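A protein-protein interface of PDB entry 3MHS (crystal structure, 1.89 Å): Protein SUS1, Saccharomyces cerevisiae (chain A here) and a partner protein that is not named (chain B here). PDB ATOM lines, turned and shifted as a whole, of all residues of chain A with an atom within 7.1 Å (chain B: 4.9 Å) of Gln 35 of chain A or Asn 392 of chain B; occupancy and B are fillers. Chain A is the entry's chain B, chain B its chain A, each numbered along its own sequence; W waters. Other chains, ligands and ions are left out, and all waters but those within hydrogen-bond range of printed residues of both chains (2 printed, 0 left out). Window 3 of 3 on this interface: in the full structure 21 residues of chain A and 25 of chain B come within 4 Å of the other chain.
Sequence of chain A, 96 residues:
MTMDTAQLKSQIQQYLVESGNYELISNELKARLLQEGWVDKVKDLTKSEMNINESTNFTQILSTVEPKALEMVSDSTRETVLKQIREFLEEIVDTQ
The side-chain amide nitrogen (ND2) of Asn 392 of chain B sits at hydrogen-bond distance from the side-chain amide oxygen (OE1) of Gln 35 of chain A, 3.3 Å away.
N of Asn 392 of chain B is in hydrogen-bond range of OH of Tyr 322 of chain B, 2.9 Å away.
O of Ala 31 of chain A lies within hydrogen-bond range of NE2 of Gln 35 of chain A, at 3.0 Å.
OD1 of Asn 392 of chain B sits at hydrogen-bond distance from N of Lys 394 of chain B, 3.1 Å away.
The side-chain carboxylate (OD1) of Asp 413 of chain B lies within salt-bridge range of the side-chain amino group (NZ) of Lys 394 of chain B (2.8 Å).
OD1 of Asn 392 of chain B sits at hydrogen-bond distance from N of Ile 414 of chain B.
ND2 of Asn 392 of chain B sits at hydrogen-bond distance from OD1 of Asp 413 of chain B.
Among the printed residues, pairs that only touch across the chains: Leu 34 of chain A with Tyr 390 of chain B, Ala 31 of chain A with Ile 415 of chain B, Ala 31 of chain A with Asp 413 of chain B, Gln 35 of chain A with Ile 415 of chain B and Leu 34 of chain A with Ile 415 of chain B.
Of the printed residues of chain B, Leu 34 of chain A touches Tyr 390 and Ile 415.
Printed residues of chain B within 4 Å of Gln 35 of chain A: Asn 392 and Ile 415.
Printed residues of chain A within 4 Å of Asn 392 of chain B: Gln 35 (3.3 Å).
Of the printed residues of chain A, Asp 413 of chain B touches Ala 31.
Of the printed residues of chain A, Ile 415 of chain B touches Ala 31 (3.5 Å), Leu 34 (3.9 Å) and Gln 35 (3.5 Å).
The nearest printed residue of chain B that does not touch Gln 35 of chain A is Tyr 390 of chain B (4.2 Å).
Hydrophobic or aromatic side chains of chain A within 4 Å of the printed part of chain B: Ala 31 and Leu 34.
Of the 12 printed residues of chain B, 4 touch a printed residue of chain A.
Printed residues of chain B that touch a printed residue of chain A: Tyr 390, Asn 392, Asp 413 and Ile 415.
Hydrophobic or aromatic side chains of chain B within 4 Å of the printed part of chain A: Tyr 390 and Ile 415.
Among the printed residues, 6 pairs touch across the chains.
Among the printed residues, no Asp or Glu carboxylate lies within 4 Å of a Lys or Arg side-chain nitrogen of the other chain.
Water W1 lies within hydrogen-bond range of OG1 of Thr 389 of chain B (2.7 Å), O of Gln 35 of chain A (3.1 Å) and N of Tyr 390 of chain B (3.1 Å).
Water W2 lies within hydrogen-bond range of OD1 of Asp 413 of chain B (2.8 Å), NE2 of Gln 35 of chain A (2.9 Å) and ND2 of Asn 392 of chain B (3.3 Å).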
ATOM      1  N   GLU A  28      -7.795  22.670 -16.330  1.00  0.00           N
ATOM      2  CA  GLU A  28      -9.234  22.891 -16.308  1.00  0.00           C
ATOM      3  C   GLU A  28      -9.585  24.364 -16.555  1.00  0.00           C
ATOM      4  O   GLU A  28     -10.532  24.647 -17.301  1.00  0.00           O
ATOM      5  CB  GLU A  28      -9.866  22.369 -15.008  1.00  0.00           C
ATOM      6  CG  GLU A  28     -10.399  20.911 -15.149  1.00  0.00           C
ATOM      7  CD  GLU A  28      -9.611  19.867 -14.369  1.00  0.00           C
ATOM      8  OE1 GLU A  28      -8.427  19.613 -14.682  1.00  0.00           O
ATOM      9  OE2 GLU A  28     -10.209  19.243 -13.470  1.00  0.00           O
ATOM     10  N   LEU A  29      -8.814  25.277 -15.966  1.00  0.00           N
ATOM     11  CA  LEU A  29      -8.964  26.722 -16.254  1.00  0.00           C
ATOM     12  C   LEU A  29      -8.810  26.999 -17.759  1.00  0.00           C
ATOM     13  O   LEU A  29      -9.661  27.648 -18.366  1.00  0.00           O
ATOM     14  CB  LEU A  29      -7.927  27.547 -15.507  1.00  0.00           C
ATOM     15  CG  LEU A  29      -7.894  29.050 -15.779  1.00  0.00           C
ATOM     16  CD1 LEU A  29      -9.240  29.708 -15.360  1.00  0.00           C
ATOM     17  CD2 LEU A  29      -6.711  29.673 -15.019  1.00  0.00           C
ATOM     18  N   LYS A  30      -7.729  26.502 -18.359  1.00  0.00           N
ATOM     19  CA  LYS A  30      -7.519  26.705 -19.784  1.00  0.00           C
ATOM     20  C   LYS A  30      -8.703  26.144 -20.603  1.00  0.00           C
ATOM     21  O   LYS A  30      -9.222  26.811 -21.484  1.00  0.00           O
ATOM     22  CB  LYS A  30      -6.201  26.065 -20.233  1.00  0.00           C
ATOM     23  CG  LYS A  30      -4.972  26.796 -19.728  1.00  0.00           C
ATOM     24  CD  LYS A  30      -3.669  26.066 -20.113  1.00  0.00           C
ATOM     25  CE  LYS A  30      -2.430  26.858 -19.707  1.00  0.00           C
ATOM     26  NZ  LYS A  30      -1.173  26.114 -20.020  1.00  0.00           N
ATOM     27  N   ALA A  31      -9.152  24.938 -20.279  1.00  0.00           N
ATOM     28  CA  ALA A  31     -10.264  24.340 -21.030  1.00  0.00           C
ATOM     29  C   ALA A  31     -11.541  25.170 -20.924  1.00  0.00           C
ATOM     30  O   ALA A  31     -12.279  25.311 -21.909  1.00  0.00           O
ATOM     31  CB  ALA A  31     -10.512  22.862 -20.599  1.00  0.00           C
ATOM     32  N   ARG A  32     -11.840  25.675 -19.731  1.00  0.00           N
ATOM     33  CA  ARG A  32     -13.045  26.462 -19.526  1.00  0.00           C
ATOM     34  C   ARG A  32     -12.997  27.747 -20.328  1.00  0.00           C
ATOM     35  O   ARG A  32     -13.967  28.098 -20.998  1.00  0.00           O
ATOM     36  CB  ARG A  32     -13.229  26.781 -18.037  1.00  0.00           C
ATOM     37  CG  ARG A  32     -13.652  25.570 -17.248  1.00  0.00           C
ATOM     38  CD  ARG A  32     -14.001  25.911 -15.780  1.00  0.00           C
ATOM     39  NE  ARG A  32     -14.384  24.666 -15.134  1.00  0.00           N
ATOM     40  CZ  ARG A  32     -15.635  24.232 -15.022  1.00  0.00           C
ATOM     41  NH1 ARG A  32     -16.655  24.969 -15.461  1.00  0.00           N
ATOM     42  NH2 ARG A  32     -15.862  23.077 -14.423  1.00  0.00           N
ATOM     43  N   LEU A  33     -11.867  28.449 -20.252  1.00  0.00           N
ATOM     44  CA  LEU A  33     -11.721  29.719 -20.935  1.00  0.00           C
ATOM     45  C   LEU A  33     -11.744  29.570 -22.446  1.00  0.00           C
ATOM     46  O   LEU A  33     -12.275  30.426 -23.163  1.00  0.00           O
ATOM     47  CB  LEU A  33     -10.429  30.390 -20.508  1.00  0.00           C
ATOM     48  CG  LEU A  33     -10.352  30.802 -19.033  1.00  0.00           C
ATOM     49  CD1 LEU A  33      -8.920  31.350 -18.702  1.00  0.00           C
ATOM     50  CD2 LEU A  33     -11.407  31.839 -18.698  1.00  0.00           C
ATOM     51  N   LEU A  34     -11.171  28.467 -22.934  1.00  0.00           N
ATOM     52  CA  LEU A  34     -11.181  28.176 -24.340  1.00  0.00           C
ATOM     53  C   LEU A  34     -12.605  27.957 -24.847  1.00  0.00           C
ATOM     54  O   LEU A  34     -13.046  28.622 -25.800  1.00  0.00           O
ATOM     55  CB  LEU A  34     -10.292  26.948 -24.596  1.00  0.00           C
ATOM     56  CG  LEU A  34     -10.092  26.463 -26.008  1.00  0.00           C
ATOM     57  CD1 LEU A  34      -9.244  27.497 -26.818  1.00  0.00           C
ATOM     58  CD2 LEU A  34      -9.468  25.063 -25.986  1.00  0.00           C
ATOM     59  N   GLN A  35     -13.343  27.075 -24.178  1.00  0.00           N
ATOM     60  CA  GLN A  35     -14.695  26.723 -24.606  1.00  0.00           C
ATOM     61  C   GLN A  35     -15.704  27.866 -24.512  1.00  0.00           C
ATOM     62  O   GLN A  35     -16.664  27.956 -25.317  1.00  0.00           O
ATOM     63  CB  GLN A  35     -15.185  25.547 -23.776  1.00  0.00           C
ATOM     64  CG  GLN A  35     -14.339  24.330 -23.938  1.00  0.00           C
ATOM     65  CD  GLN A  35     -14.809  23.213 -23.077  1.00  0.00           C
ATOM     66  OE1 GLN A  35     -15.557  22.359 -23.524  1.00  0.00           O
ATOM     67  NE2 GLN A  35     -14.423  23.232 -21.804  1.00  0.00           N
ATOM     68  N   GLU A  36     -15.528  28.747 -23.545  1.00  0.00           N
ATOM     69  CA  GLU A  36     -16.462  29.853 -23.428  1.00  0.00           C
ATOM     70  C   GLU A  36     -16.094  31.035 -24.341  1.00  0.00           C
ATOM     71  O   GLU A  36     -16.774  32.055 -24.347  1.00  0.00           O
ATOM     72  CB  GLU A  36     -16.655  30.267 -21.969  1.00  0.00           C
ATOM     73  CG  GLU A  36     -15.463  30.920 -21.307  1.00  0.00           C
ATOM     74  CD  GLU A  36     -15.576  30.917 -19.780  1.00  0.00           C
ATOM     75  OE1 GLU A  36     -16.705  30.873 -19.252  1.00  0.00           O
ATOM     76  OE2 GLU A  36     -14.530  30.958 -19.099  1.00  0.00           O
ATOM     77  N   GLY A  37     -15.056  30.863 -25.147  1.00  0.00           N
ATOM     78  CA  GLY A  37     -14.650  31.892 -26.104  1.00  0.00           C
ATOM     79  C   GLY A  37     -13.730  33.002 -25.605  1.00  0.00           C
ATOM     80  O   GLY A  37     -13.398  33.915 -26.370  1.00  0.00           O
ATOM     81  N   TRP A  38     -13.274  32.909 -24.356  1.00  0.00           N
ATOM     82  CA  TRP A  38     -12.443  33.968 -23.762  1.00  0.00           C
ATOM     83  C   TRP A  38     -11.070  34.092 -24.428  1.00  0.00           C
ATOM     84  O   TRP A  38     -10.545  35.206 -24.589  1.00  0.00           O
ATOM     85  CB  TRP A  38     -12.290  33.718 -22.260  1.00  0.00           C
ATOM     86  CG  TRP A  38     -11.408  34.676 -21.501  1.00  0.00           C
ATOM     87  CD1 TRP A  38     -11.802  35.817 -20.845  1.00  0.00           C
ATOM     88  CD2 TRP A  38     -10.000  34.551 -21.272  1.00  0.00           C
ATOM     89  NE1 TRP A  38     -10.719  36.405 -20.240  1.00  0.00           N
ATOM     90  CE2 TRP A  38      -9.609  35.634 -20.462  1.00  0.00           C
ATOM     91  CE3 TRP A  38      -9.038  33.620 -21.656  1.00  0.00           C
ATOM     92  CZ2 TRP A  38      -8.295  35.817 -20.047  1.00  0.00           C
ATOM     93  CZ3 TRP A  38      -7.731  33.800 -21.240  1.00  0.00           C
ATOM     94  CH2 TRP A  38      -7.374  34.898 -20.450  1.00  0.00           C
ATOM     95  N   VAL A  39     -10.466  32.954 -24.762  1.00  0.00           N
ATOM     96  CA  VAL A  39      -9.128  32.941 -25.383  1.00  0.00           C
ATOM     97  C   VAL A  39      -9.173  33.729 -26.680  1.00  0.00           C
ATOM     98  O   VAL A  39      -8.353  34.622 -26.923  1.00  0.00           O
ATOM     99  CB  VAL A  39      -8.608  31.503 -25.643  1.00  0.00           C
ATOM    100  CG1 VAL A  39      -7.345  31.522 -26.503  1.00  0.00           C
ATOM    101  CG2 VAL A  39      -8.386  30.786 -24.325  1.00  0.00           C
ATOM    102  N   TYR B 322     -24.554  18.780 -29.847  1.00  0.00           N
ATOM    103  CA  TYR B 322     -24.399  17.860 -28.728  1.00  0.00           C
ATOM    104  C   TYR B 322     -25.587  16.901 -28.570  1.00  0.00           C
ATOM    105  O   TYR B 322     -25.406  15.755 -28.184  1.00  0.00           O
ATOM    106  CB  TYR B 322     -24.229  18.623 -27.425  1.00  0.00           C
ATOM    107  CG  TYR B 322     -22.803  19.141 -27.214  1.00  0.00           C
ATOM    108  CD1 TYR B 322     -21.714  18.270 -27.153  1.00  0.00           C
ATOM    109  CD2 TYR B 322     -22.555  20.478 -27.110  1.00  0.00           C
ATOM    110  CE1 TYR B 322     -20.423  18.742 -26.951  1.00  0.00           C
ATOM    111  CE2 TYR B 322     -21.249  20.964 -26.903  1.00  0.00           C
ATOM    112  CZ  TYR B 322     -20.192  20.083 -26.829  1.00  0.00           C
ATOM    113  OH  TYR B 322     -18.915  20.591 -26.615  1.00  0.00           O
ATOM    114  N   THR B 389     -17.996  26.514 -31.485  1.00  0.00           N
ATOM    115  CA  THR B 389     -16.666  26.877 -31.913  1.00  0.00           C
ATOM    116  C   THR B 389     -15.625  25.909 -31.334  1.00  0.00           C
ATOM    117  O   THR B 389     -14.614  25.683 -31.942  1.00  0.00           O
ATOM    118  CB  THR B 389     -16.324  28.314 -31.502  1.00  0.00           C
ATOM    119  OG1 THR B 389     -16.584  28.453 -30.130  1.00  0.00           O
ATOM    120  CG2 THR B 389     -17.172  29.344 -32.280  1.00  0.00           C
ATOM    121  N   TYR B 390     -15.900  25.339 -30.160  1.00  0.00           N
ATOM    122  CA  TYR B 390     -15.038  24.336 -29.546  1.00  0.00           C
ATOM    123  C   TYR B 390     -15.940  23.200 -29.075  1.00  0.00           C
ATOM    124  O   TYR B 390     -16.994  23.447 -28.482  1.00  0.00           O
ATOM    125  CB  TYR B 390     -14.251  24.936 -28.403  1.00  0.00           C
ATOM    126  CG  TYR B 390     -13.237  25.908 -28.881  1.00  0.00           C
ATOM    127  CD1 TYR B 390     -11.973  25.479 -29.324  1.00  0.00           C
ATOM    128  CD2 TYR B 390     -13.525  27.268 -28.934  1.00  0.00           C
ATOM    129  CE1 TYR B 390     -11.045  26.385 -29.803  1.00  0.00           C
ATOM    130  CE2 TYR B 390     -12.584  28.196 -29.429  1.00  0.00           C
ATOM    131  CZ  TYR B 390     -11.345  27.744 -29.849  1.00  0.00           C
ATOM    132  OH  TYR B 390     -10.423  28.633 -30.370  1.00  0.00           O
ATOM    133  N   LEU B 391     -15.538  21.971 -29.372  1.00  0.00           N
ATOM    134  CA  LEU B 391     -16.364  20.772 -29.163  1.00  0.00           C
ATOM    135  C   LEU B 391     -15.654  19.889 -28.199  1.00  0.00           C
ATOM    136  O   LEU B 391     -14.498  19.543 -28.451  1.00  0.00           O
ATOM    137  CB  LEU B 391     -16.514  20.034 -30.491  1.00  0.00           C
ATOM    138  CG  LEU B 391     -17.267  18.728 -30.471  1.00  0.00           C
ATOM    139  CD1 LEU B 391     -18.698  18.959 -29.982  1.00  0.00           C
ATOM    140  CD2 LEU B 391     -17.251  18.023 -31.872  1.00  0.00           C
ATOM    141  N   ASN B 392     -16.314  19.512 -27.103  1.00  0.00           N
ATOM    142  CA  ASN B 392     -15.711  18.627 -26.128  1.00  0.00           C
ATOM    143  C   ASN B 392     -16.263  17.241 -26.374  1.00  0.00           C
ATOM    144  O   ASN B 392     -17.459  17.059 -26.295  1.00  0.00           O
ATOM    145  CB  ASN B 392     -16.050  19.089 -24.705  1.00  0.00           C
ATOM    146  CG  ASN B 392     -15.158  18.480 -23.645  1.00  0.00           C
ATOM    147  OD1 ASN B 392     -14.681  17.354 -23.780  1.00  0.00           O
ATOM    148  ND2 ASN B 392     -14.942  19.237 -22.556  1.00  0.00           N
ATOM    149  N   MET B 393     -15.385  16.268 -26.655  1.00  0.00           N
ATOM    150  CA  MET B 393     -15.837  14.916 -26.938  1.00  0.00           C
ATOM    151  C   MET B 393     -15.822  13.979 -25.761  1.00  0.00           C
ATOM    152  O   MET B 393     -16.050  12.765 -25.922  1.00  0.00           O
ATOM    153  CB  MET B 393     -15.047  14.291 -28.085  1.00  0.00           C
ATOM    154  CG  MET B 393     -15.317  14.956 -29.462  1.00  0.00           C
ATOM    155  SD  MET B 393     -17.000  14.679 -29.990  1.00  0.00           S
ATOM    156  CE  MET B 393     -16.950  12.919 -30.343  1.00  0.00           C
ATOM    157  N   LYS B 394     -15.586  14.489 -24.556  1.00  0.00           N
ATOM    158  CA  LYS B 394     -15.401  13.591 -23.421  1.00  0.00           C
ATOM    159  C   LYS B 394     -16.600  12.685 -23.087  1.00  0.00           C
ATOM    160  O   LYS B 394     -16.411  11.546 -22.699  1.00  0.00           O
ATOM    161  CB  LYS B 394     -14.960  14.338 -22.179  1.00  0.00           C
ATOM    162  CG  LYS B 394     -15.977  15.242 -21.562  1.00  0.00           C
ATOM    163  CD  LYS B 394     -15.372  15.815 -20.282  1.00  0.00           C
ATOM    164  CE  LYS B 394     -16.311  16.649 -19.508  1.00  0.00           C
ATOM    165  NZ  LYS B 394     -15.474  17.464 -18.501  1.00  0.00           N
ATOM    166  N   TYR B 396     -18.528  11.110 -25.028  1.00  0.00           N
ATOM    167  CA  TYR B 396     -18.795  10.114 -26.067  1.00  0.00           C
ATOM    168  C   TYR B 396     -17.733   9.005 -26.096  1.00  0.00           C
ATOM    169  O   TYR B 396     -17.864   8.036 -26.862  1.00  0.00           O
ATOM    170  CB  TYR B 396     -18.943  10.794 -27.444  1.00  0.00           C
ATOM    171  CG  TYR B 396     -19.916  11.912 -27.315  1.00  0.00           C
ATOM    172  CD1 TYR B 396     -21.247  11.632 -27.007  1.00  0.00           C
ATOM    173  CD2 TYR B 396     -19.491  13.234 -27.315  1.00  0.00           C
ATOM    174  CE1 TYR B 396     -22.146  12.656 -26.737  1.00  0.00           C
ATOM    175  CE2 TYR B 396     -20.378  14.277 -27.061  1.00  0.00           C
ATOM    176  CZ  TYR B 396     -21.702  13.979 -26.731  1.00  0.00           C
ATOM    177  OH  TYR B 396     -22.586  15.014 -26.493  1.00  0.00           O
ATOM    178  N   PRO B 412     -11.260  12.815 -19.289  1.00  0.00           N
ATOM    179  CA  PRO B 412     -10.831  14.192 -19.205  1.00  0.00           C
ATOM    180  C   PRO B 412     -11.371  15.022 -20.374  1.00  0.00           C
ATOM    181  O   PRO B 412     -11.878  14.448 -21.327  1.00  0.00           O
ATOM    182  CB  PRO B 412      -9.305  14.081 -19.301  1.00  0.00           C
ATOM    183  CG  PRO B 412      -9.096  12.924 -20.144  1.00  0.00           C
ATOM    184  CD  PRO B 412     -10.165  11.952 -19.795  1.00  0.00           C
ATOM    185  N   ASP B 413     -11.359  16.337 -20.242  1.00  0.00           N
ATOM    186  CA  ASP B 413     -11.750  17.206 -21.353  1.00  0.00           C
ATOM    187  C   ASP B 413     -10.895  16.873 -22.609  1.00  0.00           C
ATOM    188  O   ASP B 413      -9.665  16.729 -22.527  1.00  0.00           O
ATOM    189  CB  ASP B 413     -11.502  18.648 -21.025  1.00  0.00           C
ATOM    190  CG  ASP B 413     -12.459  19.206 -19.982  1.00  0.00           C
ATOM    191  OD1 ASP B 413     -13.648  18.885 -19.994  1.00  0.00           O
ATOM    192  OD2 ASP B 413     -11.989  19.996 -19.156  1.00  0.00           O
ATOM    193  N   ILE B 414     -11.565  16.735 -23.745  1.00  0.00           N
ATOM    194  CA  ILE B 414     -10.902  16.500 -25.005  1.00  0.00           C
ATOM    195  C   ILE B 414     -11.592  17.442 -26.000  1.00  0.00           C
ATOM    196  O   ILE B 414     -12.717  17.203 -26.468  1.00  0.00           O
ATOM    197  CB  ILE B 414     -11.007  15.031 -25.452  1.00  0.00           C
ATOM    198  CG1 ILE B 414     -10.424  14.069 -24.386  1.00  0.00           C
ATOM    199  CG2 ILE B 414     -10.241  14.860 -26.778  1.00  0.00           C
ATOM    200  CD1 ILE B 414     -10.613  12.595 -24.666  1.00  0.00           C
ATOM    201  N   ILE B 415     -10.936  18.548 -26.271  1.00  0.00           N
ATOM    202  CA  ILE B 415     -11.587  19.639 -26.960  1.00  0.00           C
ATOM    203  C   ILE B 415     -11.005  19.865 -28.340  1.00  0.00           C
ATOM    204  O   ILE B 415      -9.782  20.057 -28.504  1.00  0.00           O
ATOM    205  CB  ILE B 415     -11.432  20.929 -26.127  1.00  0.00           C
ATOM    206  CG1 ILE B 415     -12.078  20.725 -24.748  1.00  0.00           C
ATOM    207  CG2 ILE B 415     -11.988  22.181 -26.871  1.00  0.00           C
ATOM    208  CD1 ILE B 415     -11.648  21.755 -23.735  1.00  0.00           C
HETATM  209  O   HOH W   1     -17.514  26.957 -28.087  1.00  0.00           O
HETATM  210  O   HOH W   2     -15.230  21.227 -19.892  1.00  0.00           O
